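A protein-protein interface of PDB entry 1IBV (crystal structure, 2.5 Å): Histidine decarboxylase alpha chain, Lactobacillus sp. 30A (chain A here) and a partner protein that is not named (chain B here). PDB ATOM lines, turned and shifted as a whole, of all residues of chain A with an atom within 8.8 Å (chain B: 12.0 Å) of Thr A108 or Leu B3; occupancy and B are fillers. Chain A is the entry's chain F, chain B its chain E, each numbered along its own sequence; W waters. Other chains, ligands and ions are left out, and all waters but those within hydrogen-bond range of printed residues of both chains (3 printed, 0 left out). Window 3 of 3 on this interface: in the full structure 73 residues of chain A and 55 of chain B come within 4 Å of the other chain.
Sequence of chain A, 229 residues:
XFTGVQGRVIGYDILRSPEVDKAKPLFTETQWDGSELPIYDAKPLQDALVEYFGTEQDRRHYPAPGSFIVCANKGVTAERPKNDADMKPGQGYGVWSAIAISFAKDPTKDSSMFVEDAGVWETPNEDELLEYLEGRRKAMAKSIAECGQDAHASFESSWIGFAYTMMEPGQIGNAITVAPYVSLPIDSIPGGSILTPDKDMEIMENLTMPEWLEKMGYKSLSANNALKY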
ATOM      1  N   GLY A   4       0.388  13.428  22.959  1.00  0.00           N
ATOM      2  CA  GLY A   4       0.472  12.163  22.251  1.00  0.00           C
ATOM      3  C   GLY A   4       1.016  12.169  20.838  1.00  0.00           C
ATOM      4  O   GLY A   4       2.056  12.758  20.559  1.00  0.00           O
ATOM      5  N   VAL A   5       0.243  11.576  19.933  1.00  0.00           N
ATOM      6  CA  VAL A   5       0.617  11.444  18.531  1.00  0.00           C
ATOM      7  C   VAL A   5       1.019  12.729  17.812  1.00  0.00           C
ATOM      8  O   VAL A   5       1.719  12.686  16.808  1.00  0.00           O
ATOM      9  CB  VAL A   5      -0.494  10.728  17.730  1.00  0.00           C
ATOM     10  CG1 VAL A   5      -0.699   9.321  18.262  1.00  0.00           C
ATOM     11  CG2 VAL A   5      -1.790  11.507  17.805  1.00  0.00           C
ATOM     12  N   GLN A   6       0.624  13.869  18.350  1.00  0.00           N
ATOM     13  CA  GLN A   6       0.930  15.159  17.750  1.00  0.00           C
ATOM     14  C   GLN A   6       2.067  15.921  18.422  1.00  0.00           C
ATOM     15  O   GLN A   6       2.394  17.031  17.998  1.00  0.00           O
ATOM     16  CB  GLN A   6      -0.293  16.072  17.806  1.00  0.00           C
ATOM     17  CG  GLN A   6      -1.490  15.627  17.044  1.00  0.00           C
ATOM     18  CD  GLN A   6      -2.716  16.398  17.459  1.00  0.00           C
ATOM     19  OE1 GLN A   6      -3.434  15.996  18.373  1.00  0.00           O
ATOM     20  NE2 GLN A   6      -2.955  17.522  16.812  1.00  0.00           N
ATOM     21  N   GLY A   7       2.678  15.356  19.455  1.00  0.00           N
ATOM     22  CA  GLY A   7       3.704  16.121  20.133  1.00  0.00           C
ATOM     23  C   GLY A   7       5.078  15.574  20.455  1.00  0.00           C
ATOM     24  O   GLY A   7       5.374  14.381  20.349  1.00  0.00           O
ATOM     25  N   ARG A   8       5.923  16.516  20.852  1.00  0.00           N
ATOM     26  CA  ARG A   8       7.291  16.251  21.251  1.00  0.00           C
ATOM     27  C   ARG A   8       7.501  17.086  22.495  1.00  0.00           C
ATOM     28  O   ARG A   8       6.821  18.093  22.694  1.00  0.00           O
ATOM     29  CB  ARG A   8       8.263  16.689  20.169  1.00  0.00           C
ATOM     30  CG  ARG A   8       8.189  15.854  18.921  1.00  0.00           C
ATOM     31  CD  ARG A   8       9.313  16.229  18.008  1.00  0.00           C
ATOM     32  NE  ARG A   8       9.257  15.554  16.722  1.00  0.00           N
ATOM     33  CZ  ARG A   8       8.644  16.039  15.651  1.00  0.00           C
ATOM     34  NH1 ARG A   8       8.012  17.201  15.706  1.00  0.00           N
ATOM     35  NH2 ARG A   8       8.731  15.391  14.501  1.00  0.00           N
ATOM     36  N   ASP A  13      12.342  14.866  23.133  1.00  0.00           N
ATOM     37  CA  ASP A  13      12.151  14.560  21.718  1.00  0.00           C
ATOM     38  C   ASP A  13      12.947  15.486  20.814  1.00  0.00           C
ATOM     39  O   ASP A  13      13.381  15.083  19.745  1.00  0.00           O
ATOM     40  CB  ASP A  13      10.675  14.615  21.354  1.00  0.00           C
ATOM     41  CG  ASP A  13       9.877  13.517  22.013  1.00  0.00           C
ATOM     42  OD1 ASP A  13       8.986  13.833  22.819  1.00  0.00           O
ATOM     43  OD2 ASP A  13      10.138  12.337  21.714  1.00  0.00           O
ATOM     44  N   ALA A 104       5.019   7.025  26.648  1.00  0.00           N
ATOM     45  CA  ALA A 104       4.432   5.752  26.229  1.00  0.00           C
ATOM     46  C   ALA A 104       5.404   4.876  25.450  1.00  0.00           C
ATOM     47  O   ALA A 104       6.229   5.378  24.686  1.00  0.00           O
ATOM     48  CB  ALA A 104       3.187   6.011  25.404  1.00  0.00           C
ATOM     49  N   LYS A 105       5.293   3.565  25.634  1.00  0.00           N
ATOM     50  CA  LYS A 105       6.173   2.634  24.939  1.00  0.00           C
ATOM     51  C   LYS A 105       5.842   2.632  23.462  1.00  0.00           C
ATOM     52  O   LYS A 105       6.734   2.515  22.624  1.00  0.00           O
ATOM     53  CB  LYS A 105       6.040   1.217  25.507  1.00  0.00           C
ATOM     54  CG  LYS A 105       6.819   1.000  26.803  1.00  0.00           C
ATOM     55  CD  LYS A 105       6.704  -0.449  27.301  1.00  0.00           C
ATOM     56  CE  LYS A 105       7.638  -0.749  28.493  1.00  0.00           C
ATOM     57  NZ  LYS A 105       7.416  -2.132  29.014  1.00  0.00           N
ATOM     58  N   ASP A 106       4.553   2.755  23.152  1.00  0.00           N
ATOM     59  CA  ASP A 106       4.093   2.778  21.767  1.00  0.00           C
ATOM     60  C   ASP A 106       3.325   4.059  21.523  1.00  0.00           C
ATOM     61  O   ASP A 106       2.092   4.089  21.602  1.00  0.00           O
ATOM     62  CB  ASP A 106       3.196   1.569  21.449  1.00  0.00           C
ATOM     63  CG  ASP A 106       2.834   1.484  19.970  1.00  0.00           C
ATOM     64  OD1 ASP A 106       3.390   2.251  19.160  1.00  0.00           O
ATOM     65  OD2 ASP A 106       2.000   0.634  19.612  1.00  0.00           O
ATOM     66  N   PRO A 107       4.045   5.130  21.174  1.00  0.00           N
ATOM     67  CA  PRO A 107       3.454   6.440  20.910  1.00  0.00           C
ATOM     68  C   PRO A 107       2.440   6.468  19.769  1.00  0.00           C
ATOM     69  O   PRO A 107       1.855   7.514  19.507  1.00  0.00           O
ATOM     70  CB  PRO A 107       4.673   7.303  20.588  1.00  0.00           C
ATOM     71  CG  PRO A 107       5.788   6.623  21.314  1.00  0.00           C
ATOM     72  CD  PRO A 107       5.507   5.187  21.019  1.00  0.00           C
ATOM     73  N   THR A 108       2.267   5.358  19.050  1.00  0.00           N
ATOM     74  CA  THR A 108       1.295   5.345  17.965  1.00  0.00           C
ATOM     75  C   THR A 108      -0.065   4.856  18.451  1.00  0.00           C
ATOM     76  O   THR A 108      -1.074   5.051  17.784  1.00  0.00           O
ATOM     77  CB  THR A 108       1.751   4.490  16.766  1.00  0.00           C
ATOM     78  OG1 THR A 108       1.778   3.108  17.132  1.00  0.00           O
ATOM     79  CG2 THR A 108       3.123   4.918  16.298  1.00  0.00           C
ATOM     80  N   LYS A 109      -0.090   4.196  19.598  1.00  0.00           N
ATOM     81  CA  LYS A 109      -1.345   3.699  20.145  1.00  0.00           C
ATOM     82  C   LYS A 109      -1.722   4.419  21.419  1.00  0.00           C
ATOM     83  O   LYS A 109      -2.876   4.807  21.599  1.00  0.00           O
ATOM     84  CB  LYS A 109      -1.250   2.209  20.463  1.00  0.00           C
ATOM     85  CG  LYS A 109      -1.488   1.268  19.299  1.00  0.00           C
ATOM     86  CD  LYS A 109      -1.768  -0.137  19.824  1.00  0.00           C
ATOM     87  CE  LYS A 109      -0.694  -0.588  20.835  1.00  0.00           C
ATOM     88  NZ  LYS A 109      -1.180  -0.784  22.256  1.00  0.00           N
ATOM     89  N   ASP A 110      -0.745   4.582  22.309  1.00  0.00           N
ATOM     90  CA  ASP A 110      -0.981   5.227  23.598  1.00  0.00           C
ATOM     91  C   ASP A 110      -0.340   6.610  23.687  1.00  0.00           C
ATOM     92  O   ASP A 110       0.721   6.839  23.117  1.00  0.00           O
ATOM     93  CB  ASP A 110      -0.450   4.338  24.732  1.00  0.00           C
ATOM     94  CG  ASP A 110      -1.016   2.924  24.688  1.00  0.00           C
ATOM     95  OD1 ASP A 110      -2.244   2.775  24.551  1.00  0.00           O
ATOM     96  OD2 ASP A 110      -0.228   1.959  24.796  1.00  0.00           O
ATOM     97  N   SER A 111      -1.003   7.527  24.384  1.00  0.00           N
ATOM     98  CA  SER A 111      -0.481   8.876  24.556  1.00  0.00           C
ATOM     99  C   SER A 111       0.398   8.991  25.793  1.00  0.00           C
ATOM    100  O   SER A 111       0.188   8.290  26.789  1.00  0.00           O
ATOM    101  CB  SER A 111      -1.626   9.869  24.706  1.00  0.00           C
ATOM    102  OG  SER A 111      -1.134  11.169  25.004  1.00  0.00           O
ATOM    103  N   SER A 112       1.360   9.903  25.743  1.00  0.00           N
ATOM    104  CA  SER A 112       2.226  10.140  26.883  1.00  0.00           C
ATOM    105  C   SER A 112       1.345  10.904  27.855  1.00  0.00           C
ATOM    106  O   SER A 112       0.396  11.575  27.431  1.00  0.00           O
ATOM    107  CB  SER A 112       3.443  10.967  26.477  1.00  0.00           C
ATOM    108  OG  SER A 112       4.259  10.225  25.592  1.00  0.00           O
ATOM    109  N   GLU A 202      12.638  18.098  11.984  1.00  0.00           N
ATOM    110  CA  GLU A 202      13.724  17.128  11.986  1.00  0.00           C
ATOM    111  C   GLU A 202      15.039  17.722  12.446  1.00  0.00           C
ATOM    112  O   GLU A 202      15.843  17.043  13.080  1.00  0.00           O
ATOM    113  CB  GLU A 202      13.902  16.489  10.616  1.00  0.00           C
ATOM    114  CG  GLU A 202      12.752  15.571  10.244  1.00  0.00           C
ATOM    115  CD  GLU A 202      13.039  14.730   9.016  1.00  0.00           C
ATOM    116  OE1 GLU A 202      12.886  13.493   9.109  1.00  0.00           O
ATOM    117  OE2 GLU A 202      13.406  15.298   7.958  1.00  0.00           O
ATOM    118  N   GLU A 205      14.933  17.856  16.070  1.00  0.00           N
ATOM    119  CA  GLU A 205      15.016  16.514  16.626  1.00  0.00           C
ATOM    120  C   GLU A 205      16.455  16.048  16.682  1.00  0.00           C
ATOM    121  O   GLU A 205      16.850  15.356  17.609  1.00  0.00           O
ATOM    122  CB  GLU A 205      14.244  15.521  15.769  1.00  0.00           C
ATOM    123  CG  GLU A 205      12.774  15.448  16.044  1.00  0.00           C
ATOM    124  CD  GLU A 205      12.131  14.241  15.387  1.00  0.00           C
ATOM    125  OE1 GLU A 205      12.493  13.915  14.232  1.00  0.00           O
ATOM    126  OE2 GLU A 205      11.266  13.610  16.026  1.00  0.00           O
ATOM    127  N   SER B   1      11.597  11.635  12.637  1.00  0.00           N
ATOM    128  CA  SER B   1      12.172  10.345  13.097  1.00  0.00           C
ATOM    129  C   SER B   1      11.314   9.232  12.517  1.00  0.00           C
ATOM    130  O   SER B   1      10.202   9.482  12.052  1.00  0.00           O
ATOM    131  CB  SER B   1      12.136  10.276  14.623  1.00  0.00           C
ATOM    132  OG  SER B   1      10.834  10.581  15.084  1.00  0.00           O
ATOM    133  N   GLU B   2      11.805   8.002  12.600  1.00  0.00           N
ATOM    134  CA  GLU B   2      11.081   6.862  12.075  1.00  0.00           C
ATOM    135  C   GLU B   2       9.683   6.746  12.659  1.00  0.00           C
ATOM    136  O   GLU B   2       8.816   6.124  12.064  1.00  0.00           O
ATOM    137  CB  GLU B   2      11.876   5.578  12.316  1.00  0.00           C
ATOM    138  CG  GLU B   2      11.206   4.292  11.805  1.00  0.00           C
ATOM    139  CD  GLU B   2      10.784   4.342  10.324  1.00  0.00           C
ATOM    140  OE1 GLU B   2       9.791   3.656   9.969  1.00  0.00           O
ATOM    141  OE2 GLU B   2      11.438   5.051   9.512  1.00  0.00           O
ATOM    142  N   LEU B   3       9.447   7.377  13.802  1.00  0.00           N
ATOM    143  CA  LEU B   3       8.132   7.322  14.421  1.00  0.00           C
ATOM    144  C   LEU B   3       7.158   8.140  13.594  1.00  0.00           C
ATOM    145  O   LEU B   3       6.034   7.709  13.331  1.00  0.00           O
ATOM    146  CB  LEU B   3       8.185   7.868  15.849  1.00  0.00           C
ATOM    147  CG  LEU B   3       6.844   7.972  16.582  1.00  0.00           C
ATOM    148  CD1 LEU B   3       6.182   6.608  16.703  1.00  0.00           C
ATOM    149  CD2 LEU B   3       7.073   8.571  17.956  1.00  0.00           C
ATOM    150  N   ASP B   4       7.610   9.309  13.156  1.00  0.00           N
ATOM    151  CA  ASP B   4       6.776  10.198  12.360  1.00  0.00           C
ATOM    152  C   ASP B   4       6.251   9.488  11.135  1.00  0.00           C
ATOM    153  O   ASP B   4       5.098   9.660  10.774  1.00  0.00           O
ATOM    154  CB  ASP B   4       7.539  11.462  11.963  1.00  0.00           C
ATOM    155  CG  ASP B   4       7.750  12.403  13.135  1.00  0.00           C
ATOM    156  OD1 ASP B   4       6.767  13.025  13.584  1.00  0.00           O
ATOM    157  OD2 ASP B   4       8.896  12.513  13.615  1.00  0.00           O
ATOM    158  N   ALA B   5       7.078   8.634  10.546  1.00  0.00           N
ATOM    159  CA  ALA B   5       6.688   7.889   9.357  1.00  0.00           C
ATOM    160  C   ALA B   5       5.441   7.069   9.633  1.00  0.00           C
ATOM    161  O   ALA B   5       4.523   7.037   8.816  1.00  0.00           O
ATOM    162  CB  ALA B   5       7.828   6.994   8.887  1.00  0.00           C
ATOM    163  N   LYS B   6       5.403   6.424  10.794  1.00  0.00           N
ATOM    164  CA  LYS B   6       4.254   5.612  11.175  1.00  0.00           C
ATOM    165  C   LYS B   6       3.079   6.538  11.453  1.00  0.00           C
ATOM    166  O   LYS B   6       1.957   6.255  11.061  1.00  0.00           O
ATOM    167  CB  LYS B   6       4.546   4.791  12.440  1.00  0.00           C
ATOM    168  CG  LYS B   6       5.761   3.853  12.372  1.00  0.00           C
ATOM    169  CD  LYS B   6       6.138   3.379  13.789  1.00  0.00           C
ATOM    170  CE  LYS B   6       7.484   2.650  13.851  1.00  0.00           C
ATOM    171  NZ  LYS B   6       7.896   2.345  15.260  1.00  0.00           N
ATOM    172  N   LEU B   7       3.351   7.663  12.104  1.00  0.00           N
ATOM    173  CA  LEU B   7       2.307   8.623  12.447  1.00  0.00           C
ATOM    174  C   LEU B   7       1.616   9.187  11.206  1.00  0.00           C
ATOM    175  O   LEU B   7       0.387   9.282  11.141  1.00  0.00           O
ATOM    176  CB  LEU B   7       2.904   9.758  13.280  1.00  0.00           C
ATOM    177  CG  LEU B   7       2.723   9.771  14.803  1.00  0.00           C
ATOM    178  CD1 LEU B   7       2.093   8.491  15.311  1.00  0.00           C
ATOM    179  CD2 LEU B   7       4.060  10.033  15.465  1.00  0.00           C
ATOM    180  N   ASN B   8       2.419   9.562  10.224  1.00  0.00           N
ATOM    181  CA  ASN B   8       1.919  10.111   8.977  1.00  0.00           C
ATOM    182  C   ASN B   8       0.928   9.171   8.308  1.00  0.00           C
ATOM    183  O   ASN B   8      -0.095   9.608   7.802  1.00  0.00           O
ATOM    184  CB  ASN B   8       3.082  10.412   8.029  1.00  0.00           C
ATOM    185  CG  ASN B   8       3.884  11.633   8.448  1.00  0.00           C
ATOM    186  OD1 ASN B   8       5.023  11.820   8.006  1.00  0.00           O
ATOM    187  ND2 ASN B   8       3.292  12.482   9.280  1.00  0.00           N
ATOM    188  N   LYS B   9       1.205   7.874   8.341  1.00  0.00           N
ATOM    189  CA  LYS B   9       0.317   6.900   7.730  1.00  0.00           C
ATOM    190  C   LYS B   9      -1.054   6.871   8.391  1.00  0.00           C
ATOM    191  O   LYS B   9      -1.990   6.273   7.862  1.00  0.00           O
ATOM    192  CB  LYS B   9       0.960   5.514   7.733  1.00  0.00           C
ATOM    193  CG  LYS B   9       2.166   5.430   6.811  1.00  0.00           C
ATOM    194  CD  LYS B   9       2.913   4.116   6.944  1.00  0.00           C
ATOM    195  CE  LYS B   9       4.164   4.131   6.070  1.00  0.00           C
ATOM    196  NZ  LYS B   9       5.048   2.943   6.258  1.00  0.00           N
ATOM    197  N   LEU B  10      -1.175   7.529   9.535  1.00  0.00           N
ATOM    198  CA  LEU B  10      -2.439   7.595  10.256  1.00  0.00           C
ATOM    199  C   LEU B  10      -3.108   8.930   9.991  1.00  0.00           C
ATOM    200  O   LEU B  10      -4.245   9.160  10.391  1.00  0.00           O
ATOM    201  CB  LEU B  10      -2.200   7.449  11.755  1.00  0.00           C
ATOM    202  CG  LEU B  10      -1.544   6.150  12.213  1.00  0.00           C
ATOM    203  CD1 LEU B  10      -1.318   6.208  13.701  1.00  0.00           C
ATOM    204  CD2 LEU B  10      -2.419   4.964  11.858  1.00  0.00           C
ATOM    205  N   GLY B  11      -2.388   9.809   9.309  1.00  0.00           N
ATOM    206  CA  GLY B  11      -2.903  11.128   9.014  1.00  0.00           C
ATOM    207  C   GLY B  11      -2.463  12.122  10.071  1.00  0.00           C
ATOM    208  O   GLY B  11      -2.899  13.273  10.075  1.00  0.00           O
ATOM    209  N   VAL B  12      -1.574  11.685  10.955  1.00  0.00           N
ATOM    210  CA  VAL B  12      -1.072  12.536  12.027  1.00  0.00           C
ATOM    211  C   VAL B  12       0.299  13.091  11.681  1.00  0.00           C
ATOM    212  O   VAL B  12       1.087  12.426  11.009  1.00  0.00           O
ATOM    213  CB  VAL B  12      -0.922  11.742  13.342  1.00  0.00           C
ATOM    214  CG1 VAL B  12      -0.517  12.663  14.460  1.00  0.00           C
ATOM    215  CG2 VAL B  12      -2.212  11.036  13.689  1.00  0.00           C
ATOM    216  N   ASP B  13       0.578  14.310  12.121  1.00  0.00           N
ATOM    217  CA  ASP B  13       1.877  14.924  11.897  1.00  0.00           C
ATOM    218  C   ASP B  13       2.196  15.788  13.104  1.00  0.00           C
ATOM    219  O   ASP B  13       1.311  16.446  13.656  1.00  0.00           O
ATOM    220  CB  ASP B  13       1.936  15.729  10.586  1.00  0.00           C
ATOM    221  CG  ASP B  13       1.097  16.992  10.615  1.00  0.00           C
ATOM    222  OD1 ASP B  13       1.606  18.040  11.065  1.00  0.00           O
ATOM    223  OD2 ASP B  13      -0.055  16.953  10.136  1.00  0.00           O
ATOM    224  N   ARG B  14       3.459  15.789  13.512  1.00  0.00           N
ATOM    225  CA  ARG B  14       3.883  16.560  14.675  1.00  0.00           C
ATOM    226  C   ARG B  14       4.535  17.881  14.289  1.00  0.00           C
ATOM    227  O   ARG B  14       5.379  18.400  15.004  1.00  0.00           O
ATOM    228  CB  ARG B  14       4.831  15.719  15.530  1.00  0.00           C
ATOM    229  CG  ARG B  14       4.282  14.336  15.854  1.00  0.00           C
ATOM    230  CD  ARG B  14       5.043  13.674  16.973  1.00  0.00           C
ATOM    231  NE  ARG B  14       6.372  13.220  16.575  1.00  0.00           N
ATOM    232  CZ  ARG B  14       7.249  12.676  17.411  1.00  0.00           C
ATOM    233  NH1 ARG B  14       8.435  12.286  16.969  1.00  0.00           N
ATOM    234  NH2 ARG B  14       6.935  12.517  18.691  1.00  0.00           N
ATOM    235  N   ILE B  15       4.151  18.409  13.136  1.00  0.00           N
ATOM    236  CA  ILE B  15       4.693  19.673  12.656  1.00  0.00           C
ATOM    237  C   ILE B  15       4.022  20.796  13.422  1.00  0.00           C
ATOM    238  O   ILE B  15       2.800  20.825  13.525  1.00  0.00           O
ATOM    239  CB  ILE B  15       4.402  19.871  11.165  1.00  0.00           C
ATOM    240  CG1 ILE B  15       4.976  18.708  10.362  1.00  0.00           C
ATOM    241  CG2 ILE B  15       4.993  21.182  10.693  1.00  0.00           C
ATOM    242  CD1 ILE B  15       4.546  18.679   8.923  1.00  0.00           C
ATOM    243  N   TYR B  37       2.129  19.734  17.817  1.00  0.00           N
ATOM    244  CA  TYR B  37       2.470  20.641  18.898  1.00  0.00           C
ATOM    245  C   TYR B  37       3.711  20.186  19.635  1.00  0.00           C
ATOM    246  O   TYR B  37       4.107  19.022  19.540  1.00  0.00           O
ATOM    247  CB  TYR B  37       1.296  20.830  19.871  1.00  0.00           C
ATOM    248  CG  TYR B  37       0.715  19.565  20.492  1.00  0.00           C
ATOM    249  CD1 TYR B  37       1.464  18.777  21.358  1.00  0.00           C
ATOM    250  CD2 TYR B  37      -0.600  19.187  20.234  1.00  0.00           C
ATOM    251  CE1 TYR B  37       0.921  17.647  21.952  1.00  0.00           C
ATOM    252  CE2 TYR B  37      -1.153  18.056  20.822  1.00  0.00           C
ATOM    253  CZ  TYR B  37      -0.386  17.290  21.682  1.00  0.00           C
ATOM    254  OH  TYR B  37      -0.916  16.162  22.267  1.00  0.00           O
HETATM  255  O   HOH W   1       6.659  16.649  12.464  1.00  0.00           O
HETATM  256  O   HOH W   2      -1.558  14.024  19.772  1.00  0.00           O
HETATM  257  O   HOH W   3       6.019  18.081  17.563  1.00  0.00           O
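O of Val A5 touches CG of Leu B7 (3.7 Å).
Val A5 touches Val B12 (O to CG1, 3.2 Å).
Arg B14 touches Val A5 (CG to O, 3.2 Å).
Arg B14 touches Gln A6.
Gly A7 touches Tyr B37.
CD2 of Leu B3 touches CB of Pro A107, at 3.8 Å.
Thr A108 touches Leu B3.
Leu B7 touches Thr A108.
Glu A205 touches Asp B4.
Water W2 lies within hydrogen-bond range of the backbone NH (N) of Gln A6, the backbone NH (N) of Val A5 and the side-chain hydroxyl (OH) of Tyr B37.
Water W3 lies within hydrogen-bond range of O of Arg B14 (2.7 Å), NH1 of Arg A8 (2.9 Å) and O of Tyr B37 (2.9 Å).
Water W1 lies within hydrogen-bond range of N of Ile B15 (3.1 Å), NH2 of Arg A8 (3.2 Å) and O of Arg B14 (3.3 Å).
The backbone NH (N) of Ser B1 is in hydrogen-bond range of the side-chain carboxylate (OE1) of Glu A205, 2.9 Å away.
OD2 of Asp B4 is in salt-bridge range of NH2 of Arg A8 (3.0 Å).
The guanidinium group (NH2) of Arg B14 sits at hydrogen-bond distance from the backbone carbonyl oxygen (O) of Gly A7 (2.9 Å).
The backbone carbonyl oxygen (O) of Arg B14 sits at hydrogen-bond distance from the guanidinium group (NH1) of Arg A8 (3.0 Å).
The guanidinium group of Arg B14 lies within salt-bridge range of the side-chain carboxylate of Glu A205 (3.3 Å).
N of Gly A4 sits at hydrogen-bond distance from OH of Tyr B37 (3.1 Å).
The backbone carbonyl oxygen (O) of Gln A6 is in hydrogen-bond range of the backbone NH (N) of Tyr B37 (2.7 Å).
O of Tyr B37 lies within hydrogen-bond range of N of Arg A8, 3.4 Å away.
The side-chain carboxylate (OD2) of Asp B4 lies within hydrogen-bond range of the backbone NH (N) of Ser B1 (3.0 Å).
The guanidinium group (NH1) of Arg B14 is in hydrogen-bond range of the side-chain hydroxyl (OG) of Ser B1, at 3.5 Å.
The side-chain carboxylate of Asp B4 lies within salt-bridge range of the guanidinium group of Arg B14.
O of Leu B7 is in hydrogen-bond range of N of Val B12 (3.1 Å).
The side-chain amide nitrogen (ND2) of Asn B8 sits at hydrogen-bond distance from the backbone carbonyl oxygen (O) of Val B12 (2.8 Å).
OG of Ser A111 lies close to N of Gly A4, at 3.4 Å.
Of chain B, only Leu B7 (3.7 Å), Val B12 (3.2 Å) and Arg B14 (3.2 Å) come within 4 Å of Val A5.
Of the printed residues of chain B, Arg A8 touches Asp B4 (3.0 Å), Arg B14 (3.0 Å) and Tyr B37 (3.4 Å).
Asp A13 touches none of the printed residues of chain B.
No residue of chain B comes within 4 Å of Asp A106.
Pro A107 touches one residue of chain B.
Thr A108 touches two residues of chain B.
Asp A110 touches none of the printed residues of chain B.
Leu B3 touches just these residues of chain A: Pro A107 (3.8 Å) and Thr A108 (3.5 Å).
Asp B13 touches none of the printed residues of chain A.
Of the printed residues of chain A, Arg B14 touches Val A5 (3.2 Å), Gln A6 (3.7 Å), Gly A7 (2.9 Å), Arg A8 (3.0 Å) and Glu A205 (3.3 Å).
The nearest printed residue of chain A that does not touch Ser B1 is Glu A202 (4.2 Å).
Of the 16 printed residues of chain B, 7 touch a printed residue of chain A.
Printed residues of chain B that touch a printed residue of chain A: Ser B1, Leu B3, Asp B4, Leu B7, Val B12, Arg B14 and Tyr B37.
Hydrophobic or aromatic side chains of chain B that line the printed part of chain A: Leu B3, Leu B7, Val B12 and Tyr B37.
Printed residues of chain A that touch a printed residue of chain B: Gly A4, Val A5, Gln A6, Gly A7, Arg A8, Pro A107, Thr A108 and Glu A205.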
